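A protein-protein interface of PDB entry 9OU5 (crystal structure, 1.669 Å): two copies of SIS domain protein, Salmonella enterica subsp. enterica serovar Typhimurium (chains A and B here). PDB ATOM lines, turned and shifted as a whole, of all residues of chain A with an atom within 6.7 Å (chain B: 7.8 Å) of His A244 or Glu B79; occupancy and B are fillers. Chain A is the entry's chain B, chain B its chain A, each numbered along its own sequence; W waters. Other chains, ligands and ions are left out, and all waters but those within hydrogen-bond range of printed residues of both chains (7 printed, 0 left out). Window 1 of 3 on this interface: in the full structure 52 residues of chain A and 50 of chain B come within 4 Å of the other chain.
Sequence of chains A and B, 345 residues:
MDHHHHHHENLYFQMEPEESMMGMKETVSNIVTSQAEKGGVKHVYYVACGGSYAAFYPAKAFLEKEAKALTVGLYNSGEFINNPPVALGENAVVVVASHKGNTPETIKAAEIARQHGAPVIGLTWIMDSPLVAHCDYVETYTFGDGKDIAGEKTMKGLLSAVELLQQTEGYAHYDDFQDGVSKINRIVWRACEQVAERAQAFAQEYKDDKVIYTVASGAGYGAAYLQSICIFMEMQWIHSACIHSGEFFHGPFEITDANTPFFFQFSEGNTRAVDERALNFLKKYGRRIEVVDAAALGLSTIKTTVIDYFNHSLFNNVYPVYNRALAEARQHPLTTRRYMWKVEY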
ATOM      1  N   TYR A  57      10.811  14.100  15.182  1.00  0.00           N
ATOM      2  CA  TYR A  57      11.820  13.036  15.256  1.00  0.00           C
ATOM      3  C   TYR A  57      13.230  13.615  15.445  1.00  0.00           C
ATOM      4  O   TYR A  57      14.034  13.036  16.190  1.00  0.00           O
ATOM      5  CB  TYR A  57      11.725  12.156  14.001  1.00  0.00           C
ATOM      6  CG  TYR A  57      12.578  10.900  14.178  1.00  0.00           C
ATOM      7  CD1 TYR A  57      12.126   9.817  14.937  1.00  0.00           C
ATOM      8  CD2 TYR A  57      13.861  10.841  13.692  1.00  0.00           C
ATOM      9  CE1 TYR A  57      12.931   8.712  15.195  1.00  0.00           C
ATOM     10  CE2 TYR A  57      14.677   9.731  13.917  1.00  0.00           C
ATOM     11  CZ  TYR A  57      14.204   8.657  14.642  1.00  0.00           C
ATOM     12  OH  TYR A  57      15.056   7.596  14.819  1.00  0.00           O
ATOM     13  N   ALA A  61      15.928  12.378  18.259  1.00  0.00           N
ATOM     14  CA  ALA A  61      17.246  11.871  17.904  1.00  0.00           C
ATOM     15  C   ALA A  61      18.346  12.658  18.632  1.00  0.00           C
ATOM     16  O   ALA A  61      19.363  12.103  19.092  1.00  0.00           O
ATOM     17  CB  ALA A  61      17.429  11.868  16.400  1.00  0.00           C
ATOM     18  N   THR A 214      10.604   5.042   0.000  1.00  0.00           N
ATOM     19  CA  THR A 214      11.628   5.962   0.470  1.00  0.00           C
ATOM     20  C   THR A 214      12.616   5.179   1.335  1.00  0.00           C
ATOM     21  O   THR A 214      12.285   4.129   1.888  1.00  0.00           O
ATOM     22  CB  THR A 214      10.994   7.143   1.196  1.00  0.00           C
ATOM     23  OG1 THR A 214      10.363   6.677   2.377  1.00  0.00           O
ATOM     24  CG2 THR A 214      10.002   7.876   0.305  1.00  0.00           C
ATOM     25  N   VAL A 215      13.828   5.714   1.451  1.00  0.00           N
ATOM     26  CA  VAL A 215      14.899   5.103   2.225  1.00  0.00           C
ATOM     27  C   VAL A 215      15.650   6.198   2.969  1.00  0.00           C
ATOM     28  O   VAL A 215      16.048   7.187   2.351  1.00  0.00           O
ATOM     29  CB  VAL A 215      15.876   4.356   1.308  1.00  0.00           C
ATOM     30  CG1 VAL A 215      16.887   3.557   2.114  1.00  0.00           C
ATOM     31  CG2 VAL A 215      15.142   3.416   0.360  1.00  0.00           C
ATOM     32  N   ALA A 216      15.969   5.948   4.237  1.00  0.00           N
ATOM     33  CA  ALA A 216      16.718   6.913   5.032  1.00  0.00           C
ATOM     34  C   ALA A 216      17.212   6.288   6.329  1.00  0.00           C
ATOM     35  O   ALA A 216      16.759   5.216   6.734  1.00  0.00           O
ATOM     36  CB  ALA A 216      15.832   8.118   5.343  1.00  0.00           C
ATOM     37  N   SER A 217      18.039   7.046   7.053  1.00  0.00           N
ATOM     38  CA  SER A 217      18.439   6.696   8.411  1.00  0.00           C
ATOM     39  C   SER A 217      18.777   7.946   9.211  1.00  0.00           C
ATOM     40  O   SER A 217      18.969   9.008   8.641  1.00  0.00           O
ATOM     41  CB  SER A 217      19.617   5.772   8.404  1.00  0.00           C
ATOM     42  OG  SER A 217      20.769   6.399   7.848  1.00  0.00           O
ATOM     43  N   GLY A 218      18.873   7.797  10.525  1.00  0.00           N
ATOM     44  CA  GLY A 218      19.397   8.831  11.408  1.00  0.00           C
ATOM     45  C   GLY A 218      18.352   9.898  11.719  1.00  0.00           C
ATOM     46  O   GLY A 218      17.161   9.680  11.518  1.00  0.00           O
ATOM     47  N   ALA A 219      18.835  11.081  12.132  1.00  0.00           N
ATOM     48  CA  ALA A 219      17.988  12.139  12.655  1.00  0.00           C
ATOM     49  C   ALA A 219      17.047  12.744  11.605  1.00  0.00           C
ATOM     50  O   ALA A 219      16.070  13.395  11.971  1.00  0.00           O
ATOM     51  CB  ALA A 219      18.861  13.211  13.257  1.00  0.00           C
ATOM     52  N   TYR A 221      15.286  10.817   9.408  1.00  0.00           N
ATOM     53  CA  TYR A 221      14.406   9.750   8.946  1.00  0.00           C
ATOM     54  C   TYR A 221      12.950  10.210   8.821  1.00  0.00           C
ATOM     55  O   TYR A 221      12.246   9.781   7.907  1.00  0.00           O
ATOM     56  CB  TYR A 221      14.538   8.561   9.884  1.00  0.00           C
ATOM     57  CG  TYR A 221      13.595   7.442   9.521  1.00  0.00           C
ATOM     58  CD1 TYR A 221      12.330   7.401  10.084  1.00  0.00           C
ATOM     59  CD2 TYR A 221      13.958   6.416   8.630  1.00  0.00           C
ATOM     60  CE1 TYR A 221      11.425   6.412   9.743  1.00  0.00           C
ATOM     61  CE2 TYR A 221      13.066   5.395   8.309  1.00  0.00           C
ATOM     62  CZ  TYR A 221      11.804   5.399   8.878  1.00  0.00           C
ATOM     63  OH  TYR A 221      10.846   4.462   8.601  1.00  0.00           O
ATOM     64  N   CYS A 242       8.510   3.049   4.347  1.00  0.00           N
ATOM     65  CA  CYS A 242       9.657   3.925   4.467  1.00  0.00           C
ATOM     66  C   CYS A 242      10.764   3.063   5.084  1.00  0.00           C
ATOM     67  O   CYS A 242      10.652   2.642   6.221  1.00  0.00           O
ATOM     68  CB  CYS A 242       9.283   5.106   5.349  1.00  0.00           C
ATOM     69  SG  CYS A 242      10.694   6.220   5.572  1.00  0.00           S
ATOM     70  N   ILE A 243      11.775   2.718   4.303  1.00  0.00           N
ATOM     71  CA  ILE A 243      12.735   1.708   4.686  1.00  0.00           C
ATOM     72  C   ILE A 243      13.927   2.350   5.390  1.00  0.00           C
ATOM     73  O   ILE A 243      14.528   3.310   4.882  1.00  0.00           O
ATOM     74  CB  ILE A 243      13.180   0.943   3.427  1.00  0.00           C
ATOM     75  CG1 ILE A 243      11.972   0.416   2.611  1.00  0.00           C
ATOM     76  CG2 ILE A 243      14.162  -0.169   3.822  1.00  0.00           C
ATOM     77  CD1 ILE A 243      12.366  -0.063   1.223  1.00  0.00           C
ATOM     78  N   HIS A 244      14.268   1.812   6.562  1.00  0.00           N
ATOM     79  CA  HIS A 244      15.487   2.221   7.237  1.00  0.00           C
ATOM     80  C   HIS A 244      16.696   1.603   6.521  1.00  0.00           C
ATOM     81  O   HIS A 244      16.717   0.397   6.325  1.00  0.00           O
ATOM     82  CB  HIS A 244      15.397   1.857   8.714  1.00  0.00           C
ATOM     83  CG  HIS A 244      16.573   2.263   9.498  1.00  0.00           C
ATOM     84  ND1 HIS A 244      16.631   3.397  10.285  1.00  0.00           N
ATOM     85  CD2 HIS A 244      17.770   1.688   9.573  1.00  0.00           C
ATOM     86  CE1 HIS A 244      17.828   3.466  10.856  1.00  0.00           C
ATOM     87  NE2 HIS A 244      18.548   2.461  10.403  1.00  0.00           N
ATOM     88  N   SER A 245      17.679   2.450   6.170  1.00  0.00           N
ATOM     89  CA  SER A 245      18.883   2.081   5.437  1.00  0.00           C
ATOM     90  C   SER A 245      19.596   0.879   6.062  1.00  0.00           C
ATOM     91  O   SER A 245      20.226   0.101   5.361  1.00  0.00           O
ATOM     92  CB  SER A 245      19.851   3.255   5.428  1.00  0.00           C
ATOM     93  OG  SER A 245      19.300   4.313   4.668  1.00  0.00           O
ATOM     94  N   GLY A 246      19.556   0.781   7.391  1.00  0.00           N
ATOM     95  CA  GLY A 246      20.223  -0.292   8.111  1.00  0.00           C
ATOM     96  C   GLY A 246      19.482  -1.628   8.044  1.00  0.00           C
ATOM     97  O   GLY A 246      19.991  -2.653   8.516  1.00  0.00           O
ATOM     98  N   GLU A 247      18.284  -1.647   7.465  1.00  0.00           N
ATOM     99  CA  GLU A 247      17.429  -2.820   7.638  1.00  0.00           C
ATOM    100  C   GLU A 247      17.431  -3.703   6.394  1.00  0.00           C
ATOM    101  O   GLU A 247      16.896  -4.805   6.447  1.00  0.00           O
ATOM    102  CB  GLU A 247      16.036  -2.465   8.171  1.00  0.00           C
ATOM    103  CG  GLU A 247      15.987  -2.241   9.689  1.00  0.00           C
ATOM    104  CD  GLU A 247      16.368  -3.430  10.604  1.00  0.00           C
ATOM    105  OE1 GLU A 247      16.796  -3.229  11.768  1.00  0.00           O
ATOM    106  OE2 GLU A 247      16.243  -4.594  10.178  1.00  0.00           O
ATOM    107  N   PHE A 248      18.113  -3.292   5.315  1.00  0.00           N
ATOM    108  CA  PHE A 248      18.066  -4.034   4.062  1.00  0.00           C
ATOM    109  C   PHE A 248      18.760  -5.386   4.181  1.00  0.00           C
ATOM    110  O   PHE A 248      18.482  -6.295   3.403  1.00  0.00           O
ATOM    111  CB  PHE A 248      18.805  -3.366   2.894  1.00  0.00           C
ATOM    112  CG  PHE A 248      17.974  -2.328   2.168  1.00  0.00           C
ATOM    113  CD1 PHE A 248      16.949  -2.716   1.310  1.00  0.00           C
ATOM    114  CD2 PHE A 248      18.207  -0.978   2.360  1.00  0.00           C
ATOM    115  CE1 PHE A 248      16.188  -1.774   0.644  1.00  0.00           C
ATOM    116  CE2 PHE A 248      17.448  -0.039   1.688  1.00  0.00           C
ATOM    117  CZ  PHE A 248      16.442  -0.431   0.834  1.00  0.00           C
ATOM    118  N   ASN A 270      26.666  11.250  10.846  1.00  0.00           N
ATOM    119  CA  ASN A 270      27.038  10.028  11.547  1.00  0.00           C
ATOM    120  C   ASN A 270      26.385   8.785  10.944  1.00  0.00           C
ATOM    121  O   ASN A 270      26.939   7.708  11.114  1.00  0.00           O
ATOM    122  CB  ASN A 270      26.736  10.137  13.037  1.00  0.00           C
ATOM    123  CG  ASN A 270      27.647  11.111  13.759  1.00  0.00           C
ATOM    124  OD1 ASN A 270      28.861  11.058  13.587  1.00  0.00           O
ATOM    125  ND2 ASN A 270      27.099  12.069  14.481  1.00  0.00           N
ATOM    126  N   THR A 271      25.276   8.902  10.187  1.00  0.00           N
ATOM    127  CA  THR A 271      24.703   7.714   9.559  1.00  0.00           C
ATOM    128  C   THR A 271      24.916   7.723   8.037  1.00  0.00           C
ATOM    129  O   THR A 271      24.382   6.874   7.334  1.00  0.00           O
ATOM    130  CB  THR A 271      23.231   7.518   9.961  1.00  0.00           C
ATOM    131  OG1 THR A 271      22.461   8.572   9.404  1.00  0.00           O
ATOM    132  CG2 THR A 271      23.014   7.443  11.463  1.00  0.00           C
ATOM    133  N   VAL A 274      25.863   4.362   6.854  1.00  0.00           N
ATOM    134  CA  VAL A 274      24.774   3.387   6.834  1.00  0.00           C
ATOM    135  C   VAL A 274      24.020   3.544   5.514  1.00  0.00           C
ATOM    136  O   VAL A 274      23.669   2.586   4.822  1.00  0.00           O
ATOM    137  CB  VAL A 274      23.827   3.619   8.032  1.00  0.00           C
ATOM    138  CG1 VAL A 274      22.696   2.594   8.079  1.00  0.00           C
ATOM    139  CG2 VAL A 274      24.581   3.665   9.346  1.00  0.00           C
ATOM    140  N   ASP A 275      23.755   4.801   5.158  1.00  0.00           N
ATOM    141  CA  ASP A 275      23.096   5.106   3.895  1.00  0.00           C
ATOM    142  C   ASP A 275      23.907   4.617   2.677  1.00  0.00           C
ATOM    143  O   ASP A 275      23.333   4.049   1.735  1.00  0.00           O
ATOM    144  CB  ASP A 275      22.841   6.592   3.803  1.00  0.00           C
ATOM    145  CG  ASP A 275      21.804   7.148   4.779  1.00  0.00           C
ATOM    146  OD1 ASP A 275      21.086   6.336   5.388  1.00  0.00           O
ATOM    147  OD2 ASP A 275      21.784   8.400   4.972  1.00  0.00           O
ATOM    148  N   ALA A 278      23.586   0.989   1.929  1.00  0.00           N
ATOM    149  CA  ALA A 278      22.306   0.628   1.331  1.00  0.00           C
ATOM    150  C   ALA A 278      22.301   0.997  -0.153  1.00  0.00           C
ATOM    151  O   ALA A 278      21.802   0.255  -0.991  1.00  0.00           O
ATOM    152  CB  ALA A 278      21.169   1.314   2.051  1.00  0.00           C
ATOM    153  N   VAL B  47      19.459  -3.213  21.413  1.00  0.00           N
ATOM    154  CA  VAL B  47      20.111  -3.080  20.132  1.00  0.00           C
ATOM    155  C   VAL B  47      20.046  -4.411  19.388  1.00  0.00           C
ATOM    156  O   VAL B  47      20.537  -5.456  19.857  1.00  0.00           O
ATOM    157  CB  VAL B  47      21.574  -2.608  20.290  1.00  0.00           C
ATOM    158  CG1 VAL B  47      22.226  -2.334  18.953  1.00  0.00           C
ATOM    159  CG2 VAL B  47      21.680  -1.404  21.216  1.00  0.00           C
ATOM    160  N   ALA B  48      19.513  -4.343  18.182  1.00  0.00           N
ATOM    161  CA  ALA B  48      19.377  -5.505  17.317  1.00  0.00           C
ATOM    162  C   ALA B  48      18.949  -5.062  15.927  1.00  0.00           C
ATOM    163  O   ALA B  48      18.758  -3.872  15.654  1.00  0.00           O
ATOM    164  CB  ALA B  48      18.380  -6.513  17.916  1.00  0.00           C
ATOM    165  N   CYS B  49      18.873  -6.050  15.044  1.00  0.00           N
ATOM    166  CA  CYS B  49      18.435  -5.926  13.677  1.00  0.00           C
ATOM    167  C   CYS B  49      17.310  -6.910  13.427  1.00  0.00           C
ATOM    168  O   CYS B  49      17.156  -7.873  14.164  1.00  0.00           O
ATOM    169  CB  CYS B  49      19.532  -6.309  12.688  1.00  0.00           C
ATOM    170  SG  CYS B  49      20.966  -5.226  12.791  1.00  0.00           S
ATOM    171  N   TYR B  53      14.972  -6.658  16.481  1.00  0.00           N
ATOM    172  CA  TYR B  53      14.709  -5.257  16.796  1.00  0.00           C
ATOM    173  C   TYR B  53      13.236  -5.111  17.180  1.00  0.00           C
ATOM    174  O   TYR B  53      12.935  -4.584  18.233  1.00  0.00           O
ATOM    175  CB  TYR B  53      15.094  -4.405  15.583  1.00  0.00           C
ATOM    176  CG  TYR B  53      14.679  -2.948  15.710  1.00  0.00           C
ATOM    177  CD1 TYR B  53      15.495  -2.025  16.352  1.00  0.00           C
ATOM    178  CD2 TYR B  53      13.449  -2.513  15.208  1.00  0.00           C
ATOM    179  CE1 TYR B  53      15.117  -0.697  16.481  1.00  0.00           C
ATOM    180  CE2 TYR B  53      13.044  -1.194  15.351  1.00  0.00           C
ATOM    181  CZ  TYR B  53      13.896  -0.283  15.960  1.00  0.00           C
ATOM    182  OH  TYR B  53      13.524   1.014  16.104  1.00  0.00           O
ATOM    183  N   LEU B  74      15.929   2.307  21.973  1.00  0.00           N
ATOM    184  CA  LEU B  74      15.856   1.152  21.083  1.00  0.00           C
ATOM    185  C   LEU B  74      16.541   1.495  19.771  1.00  0.00           C
ATOM    186  O   LEU B  74      16.167   2.450  19.093  1.00  0.00           O
ATOM    187  CB  LEU B  74      14.389   0.746  20.871  1.00  0.00           C
ATOM    188  CG  LEU B  74      14.104  -0.283  19.786  1.00  0.00           C
ATOM    189  CD1 LEU B  74      14.771  -1.595  20.091  1.00  0.00           C
ATOM    190  CD2 LEU B  74      12.568  -0.455  19.669  1.00  0.00           C
ATOM    191  N   TYR B  75      17.553   0.714  19.391  1.00  0.00           N
ATOM    192  CA  TYR B  75      18.344   1.033  18.214  1.00  0.00           C
ATOM    193  C   TYR B  75      18.472  -0.150  17.277  1.00  0.00           C
ATOM    194  O   TYR B  75      18.640  -1.287  17.725  1.00  0.00           O
ATOM    195  CB  TYR B  75      19.785   1.402  18.606  1.00  0.00           C
ATOM    196  CG  TYR B  75      20.046   2.768  19.207  1.00  0.00           C
ATOM    197  CD1 TYR B  75      19.810   3.034  20.553  1.00  0.00           C
ATOM    198  CD2 TYR B  75      20.666   3.762  18.445  1.00  0.00           C
ATOM    199  CE1 TYR B  75      20.083   4.288  21.096  1.00  0.00           C
ATOM    200  CE2 TYR B  75      20.993   4.988  18.998  1.00  0.00           C
ATOM    201  CZ  TYR B  75      20.674   5.265  20.317  1.00  0.00           C
ATOM    202  OH  TYR B  75      21.048   6.461  20.879  1.00  0.00           O
ATOM    203  N   ASN B  76      18.462   0.165  15.979  1.00  0.00           N
ATOM    204  CA  ASN B  76      19.016  -0.683  14.931  1.00  0.00           C
ATOM    205  C   ASN B  76      20.530  -0.787  15.164  1.00  0.00           C
ATOM    206  O   ASN B  76      21.174   0.202  15.467  1.00  0.00           O
ATOM    207  CB  ASN B  76      18.724  -0.126  13.528  1.00  0.00           C
ATOM    208  CG  ASN B  76      19.624  -0.663  12.429  1.00  0.00           C
ATOM    209  OD1 ASN B  76      20.612  -0.023  12.040  1.00  0.00           O
ATOM    210  ND2 ASN B  76      19.304  -1.833  11.898  1.00  0.00           N
ATOM    211  N   SER B  77      21.103  -1.985  14.996  1.00  0.00           N
ATOM    212  CA  SER B  77      22.521  -2.194  15.327  1.00  0.00           C
ATOM    213  C   SER B  77      23.458  -1.317  14.485  1.00  0.00           C
ATOM    214  O   SER B  77      24.405  -0.687  15.005  1.00  0.00           O
ATOM    215  CB  SER B  77      22.866  -3.678  15.182  1.00  0.00           C
ATOM    216  OG  SER B  77      22.139  -4.470  16.105  1.00  0.00           O
ATOM    217  N   GLY B  78      23.153  -1.209  13.180  1.00  0.00           N
ATOM    218  CA  GLY B  78      23.895  -0.358  12.254  1.00  0.00           C
ATOM    219  C   GLY B  78      23.945   1.111  12.698  1.00  0.00           C
ATOM    220  O   GLY B  78      24.999   1.761  12.704  1.00  0.00           O
ATOM    221  N   GLU B  79      22.797   1.648  13.118  1.00  0.00           N
ATOM    222  CA  GLU B  79      22.748   3.027  13.594  1.00  0.00           C
ATOM    223  C   GLU B  79      23.519   3.187  14.900  1.00  0.00           C
ATOM    224  O   GLU B  79      24.232   4.167  15.105  1.00  0.00           O
ATOM    225  CB  GLU B  79      21.292   3.452  13.790  1.00  0.00           C
ATOM    226  CG  GLU B  79      21.175   4.926  14.140  1.00  0.00           C
ATOM    227  CD  GLU B  79      19.971   5.594  13.484  1.00  0.00           C
ATOM    228  OE1 GLU B  79      19.426   5.105  12.482  1.00  0.00           O
ATOM    229  OE2 GLU B  79      19.581   6.640  14.003  1.00  0.00           O
ATOM    230  N   PHE B  80      23.372   2.227  15.808  1.00  0.00           N
ATOM    231  CA  PHE B  80      24.019   2.288  17.106  1.00  0.00           C
ATOM    232  C   PHE B  80      25.541   2.341  16.977  1.00  0.00           C
ATOM    233  O   PHE B  80      26.169   3.095  17.694  1.00  0.00           O
ATOM    234  CB  PHE B  80      23.674   1.088  17.981  1.00  0.00           C
ATOM    235  CG  PHE B  80      24.211   1.084  19.409  1.00  0.00           C
ATOM    236  CD1 PHE B  80      23.560   1.768  20.436  1.00  0.00           C
ATOM    237  CD2 PHE B  80      25.328   0.310  19.743  1.00  0.00           C
ATOM    238  CE1 PHE B  80      23.985   1.706  21.744  1.00  0.00           C
ATOM    239  CE2 PHE B  80      25.771   0.256  21.056  1.00  0.00           C
ATOM    240  CZ  PHE B  80      25.101   0.932  22.061  1.00  0.00           C
ATOM    241  N   ILE B  81      26.121   1.525  16.107  1.00  0.00           N
ATOM    242  CA  ILE B  81      27.584   1.426  16.039  1.00  0.00           C
ATOM    243  C   ILE B  81      28.149   2.612  15.259  1.00  0.00           C
ATOM    244  O   ILE B  81      29.331   2.970  15.396  1.00  0.00           O
ATOM    245  CB  ILE B  81      28.031   0.086  15.426  1.00  0.00           C
ATOM    246  CG1 ILE B  81      27.660  -0.030  13.947  1.00  0.00           C
ATOM    247  CG2 ILE B  81      27.493  -1.104  16.207  1.00  0.00           C
ATOM    248  CD1 ILE B  81      27.949  -1.397  13.351  1.00  0.00           C
ATOM    249  N   ASN B  82      27.312   3.269  14.455  1.00  0.00           N
ATOM    250  CA  ASN B  82      27.771   4.401  13.677  1.00  0.00           C
ATOM    251  C   ASN B  82      27.518   5.693  14.422  1.00  0.00           C
ATOM    252  O   ASN B  82      28.162   6.701  14.134  1.00  0.00           O
ATOM    253  CB  ASN B  82      27.126   4.460  12.302  1.00  0.00           C
ATOM    254  CG  ASN B  82      27.849   3.557  11.332  1.00  0.00           C
ATOM    255  OD1 ASN B  82      28.851   3.964  10.753  1.00  0.00           O
ATOM    256  ND2 ASN B  82      27.373   2.339  11.159  1.00  0.00           N
ATOM    257  N   ASN B  83      26.544   5.682  15.334  1.00  0.00           N
ATOM    258  CA  ASN B  83      26.193   6.891  16.070  1.00  0.00           C
ATOM    259  C   ASN B  83      25.828   6.579  17.515  1.00  0.00           C
ATOM    260  O   ASN B  83      24.726   6.862  17.958  1.00  0.00           O
ATOM    261  CB  ASN B  83      25.068   7.622  15.346  1.00  0.00           C
ATOM    262  CG  ASN B  83      24.913   9.048  15.798  1.00  0.00           C
ATOM    263  OD1 ASN B  83      25.881   9.667  16.203  1.00  0.00           O
ATOM    264  ND2 ASN B  83      23.703   9.580  15.783  1.00  0.00           N
ATOM    265  N   PRO B  84      26.760   6.036  18.329  1.00  0.00           N
ATOM    266  CA  PRO B  84      26.409   5.658  19.687  1.00  0.00           C
ATOM    267  C   PRO B  84      26.117   6.851  20.580  1.00  0.00           C
ATOM    268  O   PRO B  84      26.729   7.919  20.424  1.00  0.00           O
ATOM    269  CB  PRO B  84      27.624   4.878  20.169  1.00  0.00           C
ATOM    270  CG  PRO B  84      28.756   5.331  19.246  1.00  0.00           C
ATOM    271  CD  PRO B  84      28.144   5.738  17.950  1.00  0.00           C
ATOM    272  N   PRO B  85      25.164   6.688  21.532  1.00  0.00           N
ATOM    273  CA  PRO B  85      24.786   7.773  22.414  1.00  0.00           C
ATOM    274  C   PRO B  85      25.917   8.188  23.335  1.00  0.00           C
ATOM    275  O   PRO B  85      26.631   7.289  23.800  1.00  0.00           O
ATOM    276  CB  PRO B  85      23.646   7.160  23.208  1.00  0.00           C
ATOM    277  CG  PRO B  85      23.882   5.657  23.135  1.00  0.00           C
ATOM    278  CD  PRO B  85      24.423   5.434  21.778  1.00  0.00           C
ATOM    279  N   GLU B 105      26.722  -6.503  12.750  1.00  0.00           N
ATOM    280  CA  GLU B 105      26.539  -5.193  13.384  1.00  0.00           C
ATOM    281  C   GLU B 105      26.195  -5.321  14.870  1.00  0.00           C
ATOM    282  O   GLU B 105      26.583  -4.463  15.687  1.00  0.00           O
ATOM    283  CB  GLU B 105      25.419  -4.375  12.722  1.00  0.00           C
ATOM    284  CG  GLU B 105      25.660  -4.116  11.241  1.00  0.00           C
ATOM    285  CD  GLU B 105      25.026  -5.147  10.320  1.00  0.00           C
ATOM    286  OE1 GLU B 105      25.205  -6.384  10.525  1.00  0.00           O
ATOM    287  OE2 GLU B 105      24.283  -4.673   9.409  1.00  0.00           O
ATOM    288  N   TYR B 225       4.233  -5.003  12.838  1.00  0.00           N
ATOM    289  CA  TYR B 225       5.273  -4.726  11.864  1.00  0.00           C
ATOM    290  C   TYR B 225       5.797  -6.050  11.289  1.00  0.00           C
ATOM    291  O   TYR B 225       5.987  -6.188  10.083  1.00  0.00           O
ATOM    292  CB  TYR B 225       6.358  -3.877  12.529  1.00  0.00           C
ATOM    293  CG  TYR B 225       7.387  -3.520  11.482  1.00  0.00           C
ATOM    294  CD1 TYR B 225       7.065  -2.539  10.570  1.00  0.00           C
ATOM    295  CD2 TYR B 225       8.550  -4.258  11.297  1.00  0.00           C
ATOM    296  CE1 TYR B 225       7.912  -2.220   9.532  1.00  0.00           C
ATOM    297  CE2 TYR B 225       9.425  -3.934  10.260  1.00  0.00           C
ATOM    298  CZ  TYR B 225       9.103  -2.905   9.393  1.00  0.00           C
ATOM    299  OH  TYR B 225       9.842  -2.480   8.320  1.00  0.00           O
HETATM  300  O   HOH W   1      22.736  -2.406   9.520  1.00  0.00           O
HETATM  301  O   HOH W   2      29.794   6.712  10.335  1.00  0.00           O
HETATM  302  O   HOH W   3      16.784   6.566  12.420  1.00  0.00           O
HETATM  303  O   HOH W   4      17.741   7.947  15.068  1.00  0.00           O
HETATM  304  O   HOH W   5      30.047   7.743  12.684  1.00  0.00           O
HETATM  305  O   HOH W   6       9.717   0.058   6.995  1.00  0.00           O
HETATM  306  O   HOH W   7      21.814  10.760  13.140  1.00  0.00           O
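Water W4 bridges the side-chain carboxylate of Glu B79 (2.5 Å) and the side-chain hydroxyl of Tyr A57 (2.7 Å).
Water W6 bridges the backbone carbonyl oxygen (O) of Cys A242 (2.9 Å) and the side-chain hydroxyl (OH) of Tyr B225 (2.9 Å).
Water W3 lies within hydrogen-bond range of the side-chain carboxylate (OE1) of Glu B79 (3.0 Å), the backbone NH (N) of Gly A218 (3.1 Å) and the side-chain hydroxyl (OH) of Tyr A57 (3.1 Å).
Hydrophobic or aromatic side chains of chain A that line the printed part of chain B: His A244 and Val A274.
Among the printed residues, 10 pairs touch across the chains.
Among the printed residues, no Asp or Glu carboxylate lies within 4 Å of a Lys or Arg side-chain nitrogen of the other chain.
Printed residues of chain B within 4 Å of Gly A218: Glu B79.
Tyr A221 touches none of the printed residues of chain B.
Of chain B, only Asn B76 (3.6 Å) and Glu B79 (2.8 Å) come within 4 Å of His A244.
Of the printed residues of chain B, Asn A270 touches Asn B82 and Asn B83.
Printed residues of chain A within 4 Å of Cys B49: Glu A247 (3.7 Å).
Of the printed residues of chain A, Asn B76 touches His A244 (3.6 Å), Gly A246 (3.5 Å) and Glu A247 (2.9 Å).
Of chain A, only Gly A218 and His A244 come within 4 Å of Glu B79.
The nearest residue of chain B that does not touch His A244 is Gly B78 (6.0 Å).
The nearest printed residue of chain A that does not touch Asn B82 is Thr A271 (4.9 Å).
No position is printed for both chains.
Of the 10 pairs that touch across the chains among the printed residues, none has its exchanged pair printed and touching as well.
ND2 of Asn B76 is in hydrogen-bond range of OE1 of Glu A247 (2.9 Å).
O of Asn A270 sits close to O of Asn B82 (3.4 Å).
The side-chain carboxylate (OE1) of Glu B79 lies close to a ring nitrogen (NE2) of His A244 (3.5 Å).
The backbone NH of Gly A218 sits at hydrogen-bond distance from the side-chain carboxylate of Glu B79 (3.4 Å).
OD1 of Asn B83 lies within hydrogen-bond range of ND2 of Asn A270.
SG of Cys B49 lies close to OG of Ser B77 (3.6 Å).
The side-chain amide oxygen of Asn B76 sits at hydrogen-bond distance from the backbone NH of Gly B78 (3.0 Å).
The backbone NH (N) of Glu B79 lies within hydrogen-bond range of the side-chain amide oxygen (OD1) of Asn B76 (3.0 Å).
The backbone carbonyl oxygen (O) of Gly B78 lies within hydrogen-bond range of the side-chain amide nitrogen (ND2) of Asn B82 (2.9 Å).
His A244 touches Asn B76 (NE2 to OD1, 3.6 Å).
Asn B76 touches Gly A246.
Glu A247 touches Cys B49.
Gly B78 touches Val A274.
ND2 of Asn B82 touches CG2 of Val A274, at 3.6 Å.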
